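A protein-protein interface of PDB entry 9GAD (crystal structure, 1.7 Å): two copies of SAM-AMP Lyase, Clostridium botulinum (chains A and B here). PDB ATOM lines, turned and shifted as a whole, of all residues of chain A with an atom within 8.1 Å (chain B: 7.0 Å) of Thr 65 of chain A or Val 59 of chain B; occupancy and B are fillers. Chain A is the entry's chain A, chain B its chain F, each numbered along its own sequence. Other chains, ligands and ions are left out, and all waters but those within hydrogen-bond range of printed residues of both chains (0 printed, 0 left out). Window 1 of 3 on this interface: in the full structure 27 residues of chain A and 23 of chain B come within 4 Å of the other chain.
The backbone carbonyl oxygen of Pro 74 of chain A sits at hydrogen-bond distance from the side-chain amide nitrogen of Gln 42 of chain B (3.2 Å).
The side-chain amide nitrogen (NE2) of Gln 42 of chain B lies within hydrogen-bond range of the side-chain sulfur (SG) of Cys 73 of chain A (3.7 Å).
The backbone carbonyl oxygen (O) of Ala 58 of chain B lies within hydrogen-bond range of the backbone NH (N) of Val 66 of chain A, at 2.8 Å.
The side-chain amide oxygen (OE1) of Gln 42 of chain B is in hydrogen-bond range of the backbone NH (N) of Asn 76 of chain A.
The backbone carbonyl oxygen (O) of Lys 64 of chain A lies within hydrogen-bond range of the backbone NH (N) of Ile 60 of chain B, 2.8 Å away.
The backbone carbonyl oxygen (O) of Tyr 67 of chain A sits at hydrogen-bond distance from the side-chain amide nitrogen (NE2) of Gln 42 of chain B (3.3 Å).
OG1 of Thr 65 of chain A is in hydrogen-bond range of OG1 of Thr 80 of chain A (2.9 Å).
OG1 of Thr 80 of chain A sits at hydrogen-bond distance from OG of Ser 63 of chain A, 2.8 Å away.
O of Thr 65 of chain A lies within hydrogen-bond range of SG of Cys 73 of chain A (3.5 Å).
The backbone NH (N) of Lys 61 of chain B lies within hydrogen-bond range of the backbone carbonyl oxygen (O) of Val 82 of chain B, at 2.9 Å.
The side-chain amide nitrogen (NE2) of Gln 30 of chain A is in hydrogen-bond range of the backbone carbonyl oxygen (O) of Ser 63 of chain A (3.4 Å).
The backbone NH (N) of Val 59 of chain B lies within hydrogen-bond range of the backbone carbonyl oxygen (O) of Thr 84 of chain B, 2.8 Å away.
Pro 62 of chain A touches Lys 61 of chain B (O to CG, 3.8 Å).
Ser 63 of chain A touches Val 59 of chain B.
Ile 60 of chain B touches Ser 63 of chain A (O to CA, 3.1 Å).
Lys 64 of chain A touches Ala 58 of chain B (O to O, 3.9 Å).
Lys 64 of chain A touches Val 59 of chain B (O to CA, 3.5 Å).
Ala 58 of chain B touches Thr 65 of chain A (O to CA, 3.5 Å).
Gln 42 of chain B touches Val 66 of chain A.
O of Val 66 of chain A touches CA of Ser 57 of chain B, at 3.3 Å.
Val 66 of chain A touches Ile 60 of chain B.
Glu 75 of chain A touches Gln 42 of chain B.
Of the printed residues of chain B, Thr 65 of chain A touches Ala 58 (3.5 Å) and Val 59 (3.4 Å).
Of chain A, only Ser 63 (3.7 Å), Lys 64 (3.5 Å), Thr 65 (3.4 Å) and Val 82 (3.7 Å) come within 4 Å of Val 59 of chain B.
Of chain A, only Lys 64, Thr 65 and Val 66 come within 4 Å of Ala 58 of chain B.
Of the printed residues of chain A, Lys 61 of chain B touches Pro 62 (3.8 Å).
Printed residues of chain B within 4 Å of Asn 76 of chain A: Gln 42 (2.9 Å).
Printed residues of chain B within 4 Å of Tyr 67 of chain A: Gln 42 (3.3 Å).
Ile 16 of chain A touches none of the printed residues of chain B.
The nearest residue of chain A that does not touch Val 59 of chain B is Val 17 of chain A (4.1 Å).
Printed residues of chain B that touch a printed residue of chain A: Trp 41, Gln 42, Ser 57, Ala 58, Val 59, Ile 60 and Lys 61.
Hydrophobic or aromatic side chains of chain B within 4 Å of the printed part of chain A: Trp 41, Val 59 and Ile 60.
Printed residues of chain A that touch a printed residue of chain B: Pro 62, Ser 63, Lys 64, Thr 65, Val 66, Tyr 67, Cys 73, Pro 74, Glu 75, Asn 76 and Val 82.
Among the printed residues, no Asp or Glu carboxylate lies within 4 Å of a Lys or Arg side-chain nitrogen of the other chain.
Positions printed for both chains: 15, 61 and 82.
Of the 19 pairs that touch across the chains among the printed residues, none has its exchanged pair printed and touching as well.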
ATOM      1  N   GLU A  15     -36.410 -15.662  -1.249  1.00  0.00           N
ATOM      2  CA  GLU A  15     -35.248 -16.490  -1.556  1.00  0.00           C
ATOM      3  C   GLU A  15     -34.096 -16.140  -0.614  1.00  0.00           C
ATOM      4  O   GLU A  15     -33.673 -14.955  -0.530  1.00  0.00           O
ATOM      5  CB  GLU A  15     -34.813 -16.282  -3.008  1.00  0.00           C
ATOM      6  CG  GLU A  15     -33.703 -17.236  -3.443  1.00  0.00           C
ATOM      7  CD  GLU A  15     -33.688 -17.528  -4.930  1.00  0.00           C
ATOM      8  OE1 GLU A  15     -32.702 -17.102  -5.531  1.00  0.00           O
ATOM      9  OE2 GLU A  15     -34.602 -18.198  -5.474  1.00  0.00           O
ATOM     10  N   ILE A  16     -33.537 -17.189   0.005  1.00  0.00           N
ATOM     11  CA  ILE A  16     -32.432 -17.122   0.946  1.00  0.00           C
ATOM     12  C   ILE A  16     -31.240 -17.879   0.365  1.00  0.00           C
ATOM     13  O   ILE A  16     -31.409 -18.961  -0.218  1.00  0.00           O
ATOM     14  CB  ILE A  16     -32.867 -17.721   2.309  1.00  0.00           C
ATOM     15  CG1 ILE A  16     -33.933 -16.908   3.005  1.00  0.00           C
ATOM     16  CG2 ILE A  16     -31.669 -17.970   3.217  1.00  0.00           C
ATOM     17  CD1 ILE A  16     -34.720 -17.653   4.097  1.00  0.00           C
ATOM     18  N   VAL A  17     -30.020 -17.351   0.551  1.00  0.00           N
ATOM     19  CA  VAL A  17     -28.807 -18.106   0.276  1.00  0.00           C
ATOM     20  C   VAL A  17     -28.029 -18.292   1.580  1.00  0.00           C
ATOM     21  O   VAL A  17     -27.837 -17.312   2.327  1.00  0.00           O
ATOM     22  CB  VAL A  17     -27.948 -17.410  -0.798  1.00  0.00           C
ATOM     23  CG1 VAL A  17     -26.740 -18.260  -1.153  1.00  0.00           C
ATOM     24  CG2 VAL A  17     -28.767 -17.098  -2.041  1.00  0.00           C
ATOM     25  N   SER A  18     -27.699 -19.562   1.868  1.00  0.00           N
ATOM     26  CA  SER A  18     -26.935 -19.899   3.067  1.00  0.00           C
ATOM     27  C   SER A  18     -25.721 -20.762   2.730  1.00  0.00           C
ATOM     28  O   SER A  18     -25.744 -21.607   1.839  1.00  0.00           O
ATOM     29  CB  SER A  18     -27.763 -20.586   4.104  1.00  0.00           C
ATOM     30  OG  SER A  18     -26.982 -20.855   5.264  1.00  0.00           O
ATOM     31  N   GLY A  19     -24.648 -20.551   3.480  1.00  0.00           N
ATOM     32  CA  GLY A  19     -23.548 -21.505   3.505  1.00  0.00           C
ATOM     33  C   GLY A  19     -23.944 -22.769   4.270  1.00  0.00           C
ATOM     34  O   GLY A  19     -25.058 -22.876   4.781  1.00  0.00           O
ATOM     35  N   GLN A  30     -22.314 -32.294  -2.063  1.00  0.00           N
ATOM     36  CA  GLN A  30     -23.474 -31.433  -2.267  1.00  0.00           C
ATOM     37  C   GLN A  30     -24.790 -32.170  -1.984  1.00  0.00           C
ATOM     38  O   GLN A  30     -25.731 -31.559  -1.508  1.00  0.00           O
ATOM     39  CB  GLN A  30     -23.461 -30.791  -3.652  1.00  0.00           C
ATOM     40  CG  GLN A  30     -22.370 -29.740  -3.800  1.00  0.00           C
ATOM     41  CD  GLN A  30     -22.396 -29.037  -5.132  1.00  0.00           C
ATOM     42  OE1 GLN A  30     -21.853 -29.558  -6.116  1.00  0.00           O
ATOM     43  NE2 GLN A  30     -22.960 -27.823  -5.168  1.00  0.00           N
ATOM     44  N   LYS A  61     -32.159 -25.828  -3.406  1.00  0.00           N
ATOM     45  CA  LYS A  61     -31.328 -26.151  -4.547  1.00  0.00           C
ATOM     46  C   LYS A  61     -29.857 -26.174  -4.131  1.00  0.00           C
ATOM     47  O   LYS A  61     -29.403 -25.291  -3.380  1.00  0.00           O
ATOM     48  CB  LYS A  61     -31.490 -25.147  -5.695  1.00  0.00           C
ATOM     49  CG  LYS A  61     -32.795 -25.193  -6.476  1.00  0.00           C
ATOM     50  CD  LYS A  61     -34.028 -24.661  -5.790  1.00  0.00           C
ATOM     51  CE  LYS A  61     -33.773 -23.306  -5.222  1.00  0.00           C
ATOM     52  NZ  LYS A  61     -35.021 -22.599  -4.982  1.00  0.00           N
ATOM     53  N   PRO A  62     -29.040 -27.120  -4.647  1.00  0.00           N
ATOM     54  CA  PRO A  62     -27.597 -27.068  -4.479  1.00  0.00           C
ATOM     55  C   PRO A  62     -27.000 -25.977  -5.347  1.00  0.00           C
ATOM     56  O   PRO A  62     -27.554 -25.639  -6.386  1.00  0.00           O
ATOM     57  CB  PRO A  62     -27.159 -28.479  -4.935  1.00  0.00           C
ATOM     58  CG  PRO A  62     -28.150 -28.787  -6.054  1.00  0.00           C
ATOM     59  CD  PRO A  62     -29.469 -28.223  -5.530  1.00  0.00           C
ATOM     60  N   SER A  63     -25.860 -25.424  -4.885  1.00  0.00           N
ATOM     61  CA  SER A  63     -25.233 -24.286  -5.538  1.00  0.00           C
ATOM     62  C   SER A  63     -23.811 -24.089  -5.037  1.00  0.00           C
ATOM     63  O   SER A  63     -23.391 -24.684  -4.045  1.00  0.00           O
ATOM     64  CB  SER A  63     -26.028 -23.009  -5.314  1.00  0.00           C
ATOM     65  OG  SER A  63     -26.130 -22.732  -3.918  1.00  0.00           O
ATOM     66  N   LYS A  64     -23.086 -23.200  -5.736  1.00  0.00           N
ATOM     67  CA  LYS A  64     -21.844 -22.645  -5.224  1.00  0.00           C
ATOM     68  C   LYS A  64     -21.881 -21.132  -5.398  1.00  0.00           C
ATOM     69  O   LYS A  64     -22.370 -20.642  -6.410  1.00  0.00           O
ATOM     70  CB  LYS A  64     -20.628 -23.222  -5.938  1.00  0.00           C
ATOM     71  CG  LYS A  64     -20.524 -24.767  -5.883  1.00  0.00           C
ATOM     72  CD  LYS A  64     -19.214 -25.500  -5.572  1.00  0.00           C
ATOM     73  CE  LYS A  64     -17.952 -24.717  -5.535  1.00  0.00           C
ATOM     74  NZ  LYS A  64     -16.834 -25.572  -5.890  1.00  0.00           N
ATOM     75  N   THR A  65     -21.371 -20.390  -4.413  1.00  0.00           N
ATOM     76  CA  THR A  65     -21.401 -18.939  -4.452  1.00  0.00           C
ATOM     77  C   THR A  65     -19.982 -18.391  -4.651  1.00  0.00           C
ATOM     78  O   THR A  65     -19.074 -18.735  -3.910  1.00  0.00           O
ATOM     79  CB  THR A  65     -22.061 -18.382  -3.192  1.00  0.00           C
ATOM     80  OG1 THR A  65     -23.433 -18.805  -3.205  1.00  0.00           O
ATOM     81  CG2 THR A  65     -22.093 -16.864  -3.167  1.00  0.00           C
ATOM     82  N   VAL A  66     -19.825 -17.572  -5.701  1.00  0.00           N
ATOM     83  CA  VAL A  66     -18.524 -17.027  -6.095  1.00  0.00           C
ATOM     84  C   VAL A  66     -18.440 -15.584  -5.623  1.00  0.00           C
ATOM     85  O   VAL A  66     -19.260 -14.754  -5.995  1.00  0.00           O
ATOM     86  CB  VAL A  66     -18.369 -17.113  -7.627  1.00  0.00           C
ATOM     87  CG1 VAL A  66     -17.094 -16.441  -8.143  1.00  0.00           C
ATOM     88  CG2 VAL A  66     -18.426 -18.565  -8.098  1.00  0.00           C
ATOM     89  N   TYR A  67     -17.422 -15.304  -4.792  1.00  0.00           N
ATOM     90  CA  TYR A  67     -17.110 -13.937  -4.406  1.00  0.00           C
ATOM     91  C   TYR A  67     -15.583 -13.828  -4.306  1.00  0.00           C
ATOM     92  O   TYR A  67     -14.856 -14.743  -4.691  1.00  0.00           O
ATOM     93  CB  TYR A  67     -17.916 -13.524  -3.163  1.00  0.00           C
ATOM     94  CG  TYR A  67     -17.672 -14.326  -1.896  1.00  0.00           C
ATOM     95  CD1 TYR A  67     -18.191 -15.616  -1.736  1.00  0.00           C
ATOM     96  CD2 TYR A  67     -16.908 -13.804  -0.857  1.00  0.00           C
ATOM     97  CE1 TYR A  67     -17.940 -16.359  -0.601  1.00  0.00           C
ATOM     98  CE2 TYR A  67     -16.688 -14.530   0.303  1.00  0.00           C
ATOM     99  CZ  TYR A  67     -17.197 -15.815   0.432  1.00  0.00           C
ATOM    100  OH  TYR A  67     -16.984 -16.568   1.563  1.00  0.00           O
ATOM    101  N   ASN A  68     -15.117 -12.662  -3.866  1.00  0.00           N
ATOM    102  CA  ASN A  68     -13.692 -12.342  -3.895  1.00  0.00           C
ATOM    103  C   ASN A  68     -12.939 -13.251  -2.925  1.00  0.00           C
ATOM    104  O   ASN A  68     -13.300 -13.326  -1.746  1.00  0.00           O
ATOM    105  CB  ASN A  68     -13.520 -10.867  -3.582  1.00  0.00           C
ATOM    106  CG  ASN A  68     -12.118 -10.349  -3.820  1.00  0.00           C
ATOM    107  OD1 ASN A  68     -11.155 -11.119  -3.970  1.00  0.00           O
ATOM    108  ND2 ASN A  68     -12.008  -9.039  -3.784  1.00  0.00           N
ATOM    109  N   CYS A  73     -13.527 -16.329   0.076  1.00  0.00           N
ATOM    110  CA  CYS A  73     -14.155 -17.300  -0.813  1.00  0.00           C
ATOM    111  C   CYS A  73     -13.120 -18.337  -1.227  1.00  0.00           C
ATOM    112  O   CYS A  73     -12.021 -17.963  -1.633  1.00  0.00           O
ATOM    113  CB  CYS A  73     -14.763 -16.657  -2.055  1.00  0.00           C
ATOM    114  SG  CYS A  73     -15.809 -17.776  -3.024  1.00  0.00           S
ATOM    115  N   PRO A  74     -13.417 -19.651  -1.158  1.00  0.00           N
ATOM    116  CA  PRO A  74     -12.543 -20.655  -1.760  1.00  0.00           C
ATOM    117  C   PRO A  74     -12.419 -20.484  -3.271  1.00  0.00           C
ATOM    118  O   PRO A  74     -13.305 -19.910  -3.917  1.00  0.00           O
ATOM    119  CB  PRO A  74     -13.191 -22.006  -1.410  1.00  0.00           C
ATOM    120  CG  PRO A  74     -14.162 -21.707  -0.300  1.00  0.00           C
ATOM    121  CD  PRO A  74     -14.561 -20.257  -0.458  1.00  0.00           C
ATOM    122  N   GLU A  75     -11.323 -21.029  -3.822  1.00  0.00           N
ATOM    123  CA  GLU A  75     -11.140 -21.104  -5.261  1.00  0.00           C
ATOM    124  C   GLU A  75     -12.321 -21.850  -5.881  1.00  0.00           C
ATOM    125  O   GLU A  75     -12.656 -22.940  -5.434  1.00  0.00           O
ATOM    126  CB  GLU A  75      -9.801 -21.772  -5.595  1.00  0.00           C
ATOM    127  CG  GLU A  75      -9.484 -21.720  -7.087  1.00  0.00           C
ATOM    128  CD  GLU A  75      -8.326 -22.568  -7.577  1.00  0.00           C
ATOM    129  OE1 GLU A  75      -8.024 -22.334  -8.758  1.00  0.00           O
ATOM    130  OE2 GLU A  75      -7.768 -23.441  -6.868  1.00  0.00           O
ATOM    131  N   ASN A  76     -12.957 -21.232  -6.895  1.00  0.00           N
ATOM    132  CA  ASN A  76     -14.061 -21.813  -7.654  1.00  0.00           C
ATOM    133  C   ASN A  76     -15.415 -21.675  -6.947  1.00  0.00           C
ATOM    134  O   ASN A  76     -16.419 -22.067  -7.519  1.00  0.00           O
ATOM    135  CB  ASN A  76     -13.861 -23.288  -8.013  1.00  0.00           C
ATOM    136  CG  ASN A  76     -12.615 -23.526  -8.836  1.00  0.00           C
ATOM    137  OD1 ASN A  76     -12.133 -22.608  -9.513  1.00  0.00           O
ATOM    138  ND2 ASN A  76     -12.094 -24.747  -8.793  1.00  0.00           N
ATOM    139  N   GLY A  77     -15.446 -21.108  -5.732  1.00  0.00           N
ATOM    140  CA  GLY A  77     -16.698 -20.764  -5.055  1.00  0.00           C
ATOM    141  C   GLY A  77     -16.913 -21.583  -3.781  1.00  0.00           C
ATOM    142  O   GLY A  77     -16.298 -22.632  -3.590  1.00  0.00           O
ATOM    143  N   GLU A  78     -17.810 -21.079  -2.923  1.00  0.00           N
ATOM    144  CA  GLU A  78     -18.182 -21.698  -1.654  1.00  0.00           C
ATOM    145  C   GLU A  78     -19.469 -22.511  -1.815  1.00  0.00           C
ATOM    146  O   GLU A  78     -20.412 -22.032  -2.424  1.00  0.00           O
ATOM    147  CB  GLU A  78     -18.416 -20.556  -0.661  1.00  0.00           C
ATOM    148  CG  GLU A  78     -18.813 -21.060   0.714  1.00  0.00           C
ATOM    149  CD  GLU A  78     -18.892 -20.083   1.858  1.00  0.00           C
ATOM    150  OE1 GLU A  78     -19.645 -20.430   2.803  1.00  0.00           O
ATOM    151  OE2 GLU A  78     -18.153 -19.080   1.838  1.00  0.00           O
ATOM    152  N   GLU A  79     -19.503 -23.719  -1.227  1.00  0.00           N
ATOM    153  CA  GLU A  79     -20.700 -24.561  -1.283  1.00  0.00           C
ATOM    154  C   GLU A  79     -21.854 -23.883  -0.530  1.00  0.00           C
ATOM    155  O   GLU A  79     -21.730 -23.509   0.633  1.00  0.00           O
ATOM    156  CB  GLU A  79     -20.318 -25.937  -0.728  1.00  0.00           C
ATOM    157  CG  GLU A  79     -21.390 -26.999  -0.922  1.00  0.00           C
ATOM    158  CD  GLU A  79     -20.902 -28.422  -0.635  1.00  0.00           C
ATOM    159  OE1 GLU A  79     -19.762 -28.802  -1.004  1.00  0.00           O
ATOM    160  OE2 GLU A  79     -21.690 -29.149  -0.001  1.00  0.00           O
ATOM    161  N   THR A  80     -23.014 -23.760  -1.176  1.00  0.00           N
ATOM    162  CA  THR A  80     -24.166 -23.043  -0.630  1.00  0.00           C
ATOM    163  C   THR A  80     -25.460 -23.784  -1.000  1.00  0.00           C
ATOM    164  O   THR A  80     -25.475 -24.672  -1.843  1.00  0.00           O
ATOM    165  CB  THR A  80     -24.219 -21.588  -1.100  1.00  0.00           C
ATOM    166  OG1 THR A  80     -24.051 -21.503  -2.516  1.00  0.00           O
ATOM    167  CG2 THR A  80     -23.156 -20.718  -0.466  1.00  0.00           C
ATOM    168  N   VAL A  81     -26.545 -23.411  -0.325  1.00  0.00           N
ATOM    169  CA  VAL A  81     -27.899 -23.853  -0.624  1.00  0.00           C
ATOM    170  C   VAL A  81     -28.798 -22.631  -0.822  1.00  0.00           C
ATOM    171  O   VAL A  81     -28.702 -21.651  -0.079  1.00  0.00           O
ATOM    172  CB  VAL A  81     -28.458 -24.809   0.452  1.00  0.00           C
ATOM    173  CG1 VAL A  81     -29.921 -25.151   0.218  1.00  0.00           C
ATOM    174  CG2 VAL A  81     -27.639 -26.104   0.539  1.00  0.00           C
ATOM    175  N   VAL A  82     -29.679 -22.691  -1.829  1.00  0.00           N
ATOM    176  CA  VAL A  82     -30.670 -21.641  -2.089  1.00  0.00           C
ATOM    177  C   VAL A  82     -32.050 -22.157  -1.683  1.00  0.00           C
ATOM    178  O   VAL A  82     -32.421 -23.265  -2.114  1.00  0.00           O
ATOM    179  CB  VAL A  82     -30.695 -21.264  -3.583  1.00  0.00           C
ATOM    180  CG1 VAL A  82     -31.766 -20.227  -3.918  1.00  0.00           C
ATOM    181  CG2 VAL A  82     -29.320 -20.838  -4.090  1.00  0.00           C
ATOM    182  N   THR A 119     -28.538 -13.485   3.188  1.00  0.00           N
ATOM    183  CA  THR A 119     -29.452 -12.681   2.377  1.00  0.00           C
ATOM    184  C   THR A 119     -30.833 -13.329   2.345  1.00  0.00           C
ATOM    185  O   THR A 119     -30.954 -14.566   2.260  1.00  0.00           O
ATOM    186  CB  THR A 119     -28.952 -12.504   0.940  1.00  0.00           C
ATOM    187  OG1 THR A 119     -28.797 -13.804   0.337  1.00  0.00           O
ATOM    188  CG2 THR A 119     -27.660 -11.701   0.882  1.00  0.00           C
ATOM    189  N   GLU A 121     -34.393 -12.250   0.106  1.00  0.00           N
ATOM    190  CA  GLU A 121     -35.047 -11.376  -0.860  1.00  0.00           C
ATOM    191  C   GLU A 121     -36.529 -11.681  -0.946  1.00  0.00           C
ATOM    192  O   GLU A 121     -36.904 -12.849  -0.823  1.00  0.00           O
ATOM    193  CB  GLU A 121     -34.457 -11.549  -2.253  1.00  0.00           C
ATOM    194  CG  GLU A 121     -33.026 -11.034  -2.401  1.00  0.00           C
ATOM    195  CD  GLU A 121     -32.395 -11.479  -3.698  1.00  0.00           C
ATOM    196  OE1 GLU A 121     -32.897 -11.012  -4.752  1.00  0.00           O
ATOM    197  OE2 GLU A 121     -31.466 -12.312  -3.633  1.00  0.00           O
ATOM    198  N   PHE B  14     -29.894 -10.076 -10.979  1.00  0.00           N
ATOM    199  CA  PHE B  14     -29.713 -10.592 -12.324  1.00  0.00           C
ATOM    200  C   PHE B  14     -29.734 -12.117 -12.308  1.00  0.00           C
ATOM    201  O   PHE B  14     -29.416 -12.748 -11.287  1.00  0.00           O
ATOM    202  CB  PHE B  14     -28.393 -10.110 -12.933  1.00  0.00           C
ATOM    203  CG  PHE B  14     -27.133 -10.776 -12.404  1.00  0.00           C
ATOM    204  CD1 PHE B  14     -26.680 -11.995 -12.902  1.00  0.00           C
ATOM    205  CD2 PHE B  14     -26.394 -10.188 -11.381  1.00  0.00           C
ATOM    206  CE1 PHE B  14     -25.531 -12.583 -12.401  1.00  0.00           C
ATOM    207  CE2 PHE B  14     -25.260 -10.783 -10.877  1.00  0.00           C
ATOM    208  CZ  PHE B  14     -24.824 -11.980 -11.397  1.00  0.00           C
ATOM    209  N   GLU B  15     -30.089 -12.698 -13.459  1.00  0.00           N
ATOM    210  CA  GLU B  15     -29.966 -14.127 -13.685  1.00  0.00           C
ATOM    211  C   GLU B  15     -29.519 -14.396 -15.132  1.00  0.00           C
ATOM    212  O   GLU B  15     -30.161 -13.914 -16.064  1.00  0.00           O
ATOM    213  CB  GLU B  15     -31.303 -14.834 -13.430  1.00  0.00           C
ATOM    214  CG  GLU B  15     -31.197 -16.347 -13.465  1.00  0.00           C
ATOM    215  CD  GLU B  15     -32.203 -17.077 -12.569  1.00  0.00           C
ATOM    216  OE1 GLU B  15     -33.060 -17.793 -13.100  1.00  0.00           O
ATOM    217  OE2 GLU B  15     -32.100 -16.961 -11.342  1.00  0.00           O
ATOM    218  N   TRP B  41     -15.967 -17.397 -13.739  1.00  0.00           N
ATOM    219  CA  TRP B  41     -16.657 -16.205 -13.257  1.00  0.00           C
ATOM    220  C   TRP B  41     -15.792 -15.453 -12.240  1.00  0.00           C
ATOM    221  O   TRP B  41     -15.729 -14.227 -12.244  1.00  0.00           O
ATOM    222  CB  TRP B  41     -18.040 -16.565 -12.671  1.00  0.00           C
ATOM    223  CG  TRP B  41     -18.824 -15.343 -12.286  1.00  0.00           C
ATOM    224  CD1 TRP B  41     -18.840 -14.740 -11.068  1.00  0.00           C
ATOM    225  CD2 TRP B  41     -19.615 -14.519 -13.155  1.00  0.00           C
ATOM    226  NE1 TRP B  41     -19.598 -13.603 -11.108  1.00  0.00           N
ATOM    227  CE2 TRP B  41     -20.090 -13.438 -12.376  1.00  0.00           C
ATOM    228  CE3 TRP B  41     -19.986 -14.581 -14.507  1.00  0.00           C
ATOM    229  CZ2 TRP B  41     -20.906 -12.445 -12.908  1.00  0.00           C
ATOM    230  CZ3 TRP B  41     -20.761 -13.577 -15.043  1.00  0.00           C
ATOM    231  CH2 TRP B  41     -21.203 -12.515 -14.250  1.00  0.00           C
ATOM    232  N   GLN B  42     -15.148 -16.175 -11.329  1.00  0.00           N
ATOM    233  CA  GLN B  42     -14.317 -15.562 -10.303  1.00  0.00           C
ATOM    234  C   GLN B  42     -13.220 -14.716 -10.958  1.00  0.00           C
ATOM    235  O   GLN B  42     -12.972 -13.604 -10.516  1.00  0.00           O
ATOM    236  CB  GLN B  42     -13.778 -16.680  -9.414  1.00  0.00           C
ATOM    237  CG  GLN B  42     -13.274 -16.253  -8.051  1.00  0.00           C
ATOM    238  CD  GLN B  42     -13.044 -17.461  -7.157  1.00  0.00           C
ATOM    239  OE1 GLN B  42     -12.404 -18.433  -7.563  1.00  0.00           O
ATOM    240  NE2 GLN B  42     -13.561 -17.457  -5.937  1.00  0.00           N
ATOM    241  N   SER B  57     -20.680 -10.629  -7.500  1.00  0.00           N
ATOM    242  CA  SER B  57     -20.788 -11.976  -6.978  1.00  0.00           C
ATOM    243  C   SER B  57     -21.958 -12.708  -7.644  1.00  0.00           C
ATOM    244  O   SER B  57     -22.895 -12.062  -8.120  1.00  0.00           O
ATOM    245  CB  SER B  57     -20.963 -11.943  -5.478  1.00  0.00           C
ATOM    246  OG  SER B  57     -22.075 -11.128  -5.111  1.00  0.00           O
ATOM    247  N   ALA B  58     -21.873 -14.048  -7.683  1.00  0.00           N
ATOM    248  CA  ALA B  58     -22.913 -14.887  -8.265  1.00  0.00           C
ATOM    249  C   ALA B  58     -23.066 -16.210  -7.499  1.00  0.00           C
ATOM    250  O   ALA B  58     -22.094 -16.825  -7.089  1.00  0.00           O
ATOM    251  CB  ALA B  58     -22.582 -15.166  -9.712  1.00  0.00           C
ATOM    252  N   VAL B  59     -24.318 -16.650  -7.370  1.00  0.00           N
ATOM    253  CA  VAL B  59     -24.661 -17.987  -6.913  1.00  0.00           C
ATOM    254  C   VAL B  59     -24.961 -18.826  -8.172  1.00  0.00           C
ATOM    255  O   VAL B  59     -25.777 -18.389  -8.962  1.00  0.00           O
ATOM    256  CB  VAL B  59     -25.890 -17.944  -5.992  1.00  0.00           C
ATOM    257  CG1 VAL B  59     -26.171 -19.339  -5.411  1.00  0.00           C
ATOM    258  CG2 VAL B  59     -25.753 -16.909  -4.889  1.00  0.00           C
ATOM    259  N   ILE B  60     -24.362 -20.004  -8.271  1.00  0.00           N
ATOM    260  CA  ILE B  60     -24.401 -20.802  -9.496  1.00  0.00           C
ATOM    261  C   ILE B  60     -25.079 -22.143  -9.179  1.00  0.00           C
ATOM    262  O   ILE B  60     -24.695 -22.831  -8.226  1.00  0.00           O
ATOM    263  CB  ILE B  60     -22.982 -20.981 -10.068  1.00  0.00           C
ATOM    264  CG1 ILE B  60     -22.218 -19.657 -10.276  1.00  0.00           C
ATOM    265  CG2 ILE B  60     -23.017 -21.801 -11.356  1.00  0.00           C
ATOM    266  CD1 ILE B  60     -20.767 -19.865 -10.686  1.00  0.00           C
ATOM    267  N   LYS B  61     -26.033 -22.531 -10.033  1.00  0.00           N
ATOM    268  CA  LYS B  61     -26.876 -23.703  -9.816  1.00  0.00           C
ATOM    269  C   LYS B  61     -26.825 -24.624 -11.038  1.00  0.00           C
ATOM    270  O   LYS B  61     -26.837 -24.152 -12.175  1.00  0.00           O
ATOM    271  CB  LYS B  61     -28.347 -23.338  -9.588  1.00  0.00           C
ATOM    272  CG  LYS B  61     -28.682 -22.609  -8.296  1.00  0.00           C
ATOM    273  CD  LYS B  61     -30.143 -22.222  -8.333  1.00  0.00           C
ATOM    274  CE  LYS B  61     -30.376 -21.221  -9.441  1.00  0.00           C
ATOM    275  NZ  LYS B  61     -31.803 -20.971  -9.533  1.00  0.00           N
ATOM    276  N   VAL B  82     -27.051 -21.838 -14.133  1.00  0.00           N
ATOM    277  CA  VAL B  82     -27.763 -20.599 -13.877  1.00  0.00           C
ATOM    278  C   VAL B  82     -26.979 -19.789 -12.839  1.00  0.00           C
ATOM    279  O   VAL B  82     -26.616 -20.330 -11.789  1.00  0.00           O
ATOM    280  CB  VAL B  82     -29.177 -20.900 -13.324  1.00  0.00           C
ATOM    281  CG1 VAL B  82     -29.929 -19.628 -12.992  1.00  0.00           C
ATOM    282  CG2 VAL B  82     -29.982 -21.828 -14.241  1.00  0.00           C
ATOM    283  N   LEU B  83     -26.639 -18.538 -13.174  1.00  0.00           N
ATOM    284  CA  LEU B  83     -25.906 -17.640 -12.285  1.00  0.00           C
ATOM    285  C   LEU B  83     -26.827 -16.496 -11.857  1.00  0.00           C
ATOM    286  O   LEU B  83     -27.402 -15.816 -12.698  1.00  0.00           O
ATOM    287  CB  LEU B  83     -24.674 -17.052 -12.986  1.00  0.00           C
ATOM    288  CG  LEU B  83     -23.651 -18.042 -13.538  1.00  0.00           C
ATOM    289  CD1 LEU B  83     -24.003 -18.457 -14.982  1.00  0.00           C
ATOM    290  CD2 LEU B  83     -22.237 -17.418 -13.477  1.00  0.00           C
ATOM    291  N   THR B  84     -26.901 -16.231 -10.532  1.00  0.00           N
ATOM    292  CA  THR B  84     -27.792 -15.224 -10.005  1.00  0.00           C
ATOM    293  C   THR B  84     -27.057 -14.360  -8.987  1.00  0.00           C
ATOM    294  O   THR B  84     -26.332 -14.907  -8.128  1.00  0.00           O
ATOM    295  CB  THR B  84     -28.988 -15.951  -9.344  1.00  0.00           C
ATOM    296  OG1 THR B  84     -29.603 -16.835 -10.295  1.00  0.00           O
ATOM    297  CG2 THR B  84     -30.077 -14.985  -8.935  1.00  0.00           C
ATOM    298  N   GLY B  85     -27.279 -13.039  -9.060  1.00  0.00           N
ATOM    299  CA  GLY B  85     -26.657 -12.116  -8.102  1.00  0.00           C
ATOM    300  C   GLY B  85     -27.504 -10.886  -7.872  1.00  0.00           C
ATOM    301  O   GLY B  85     -28.567 -10.744  -8.476  1.00  0.00           O
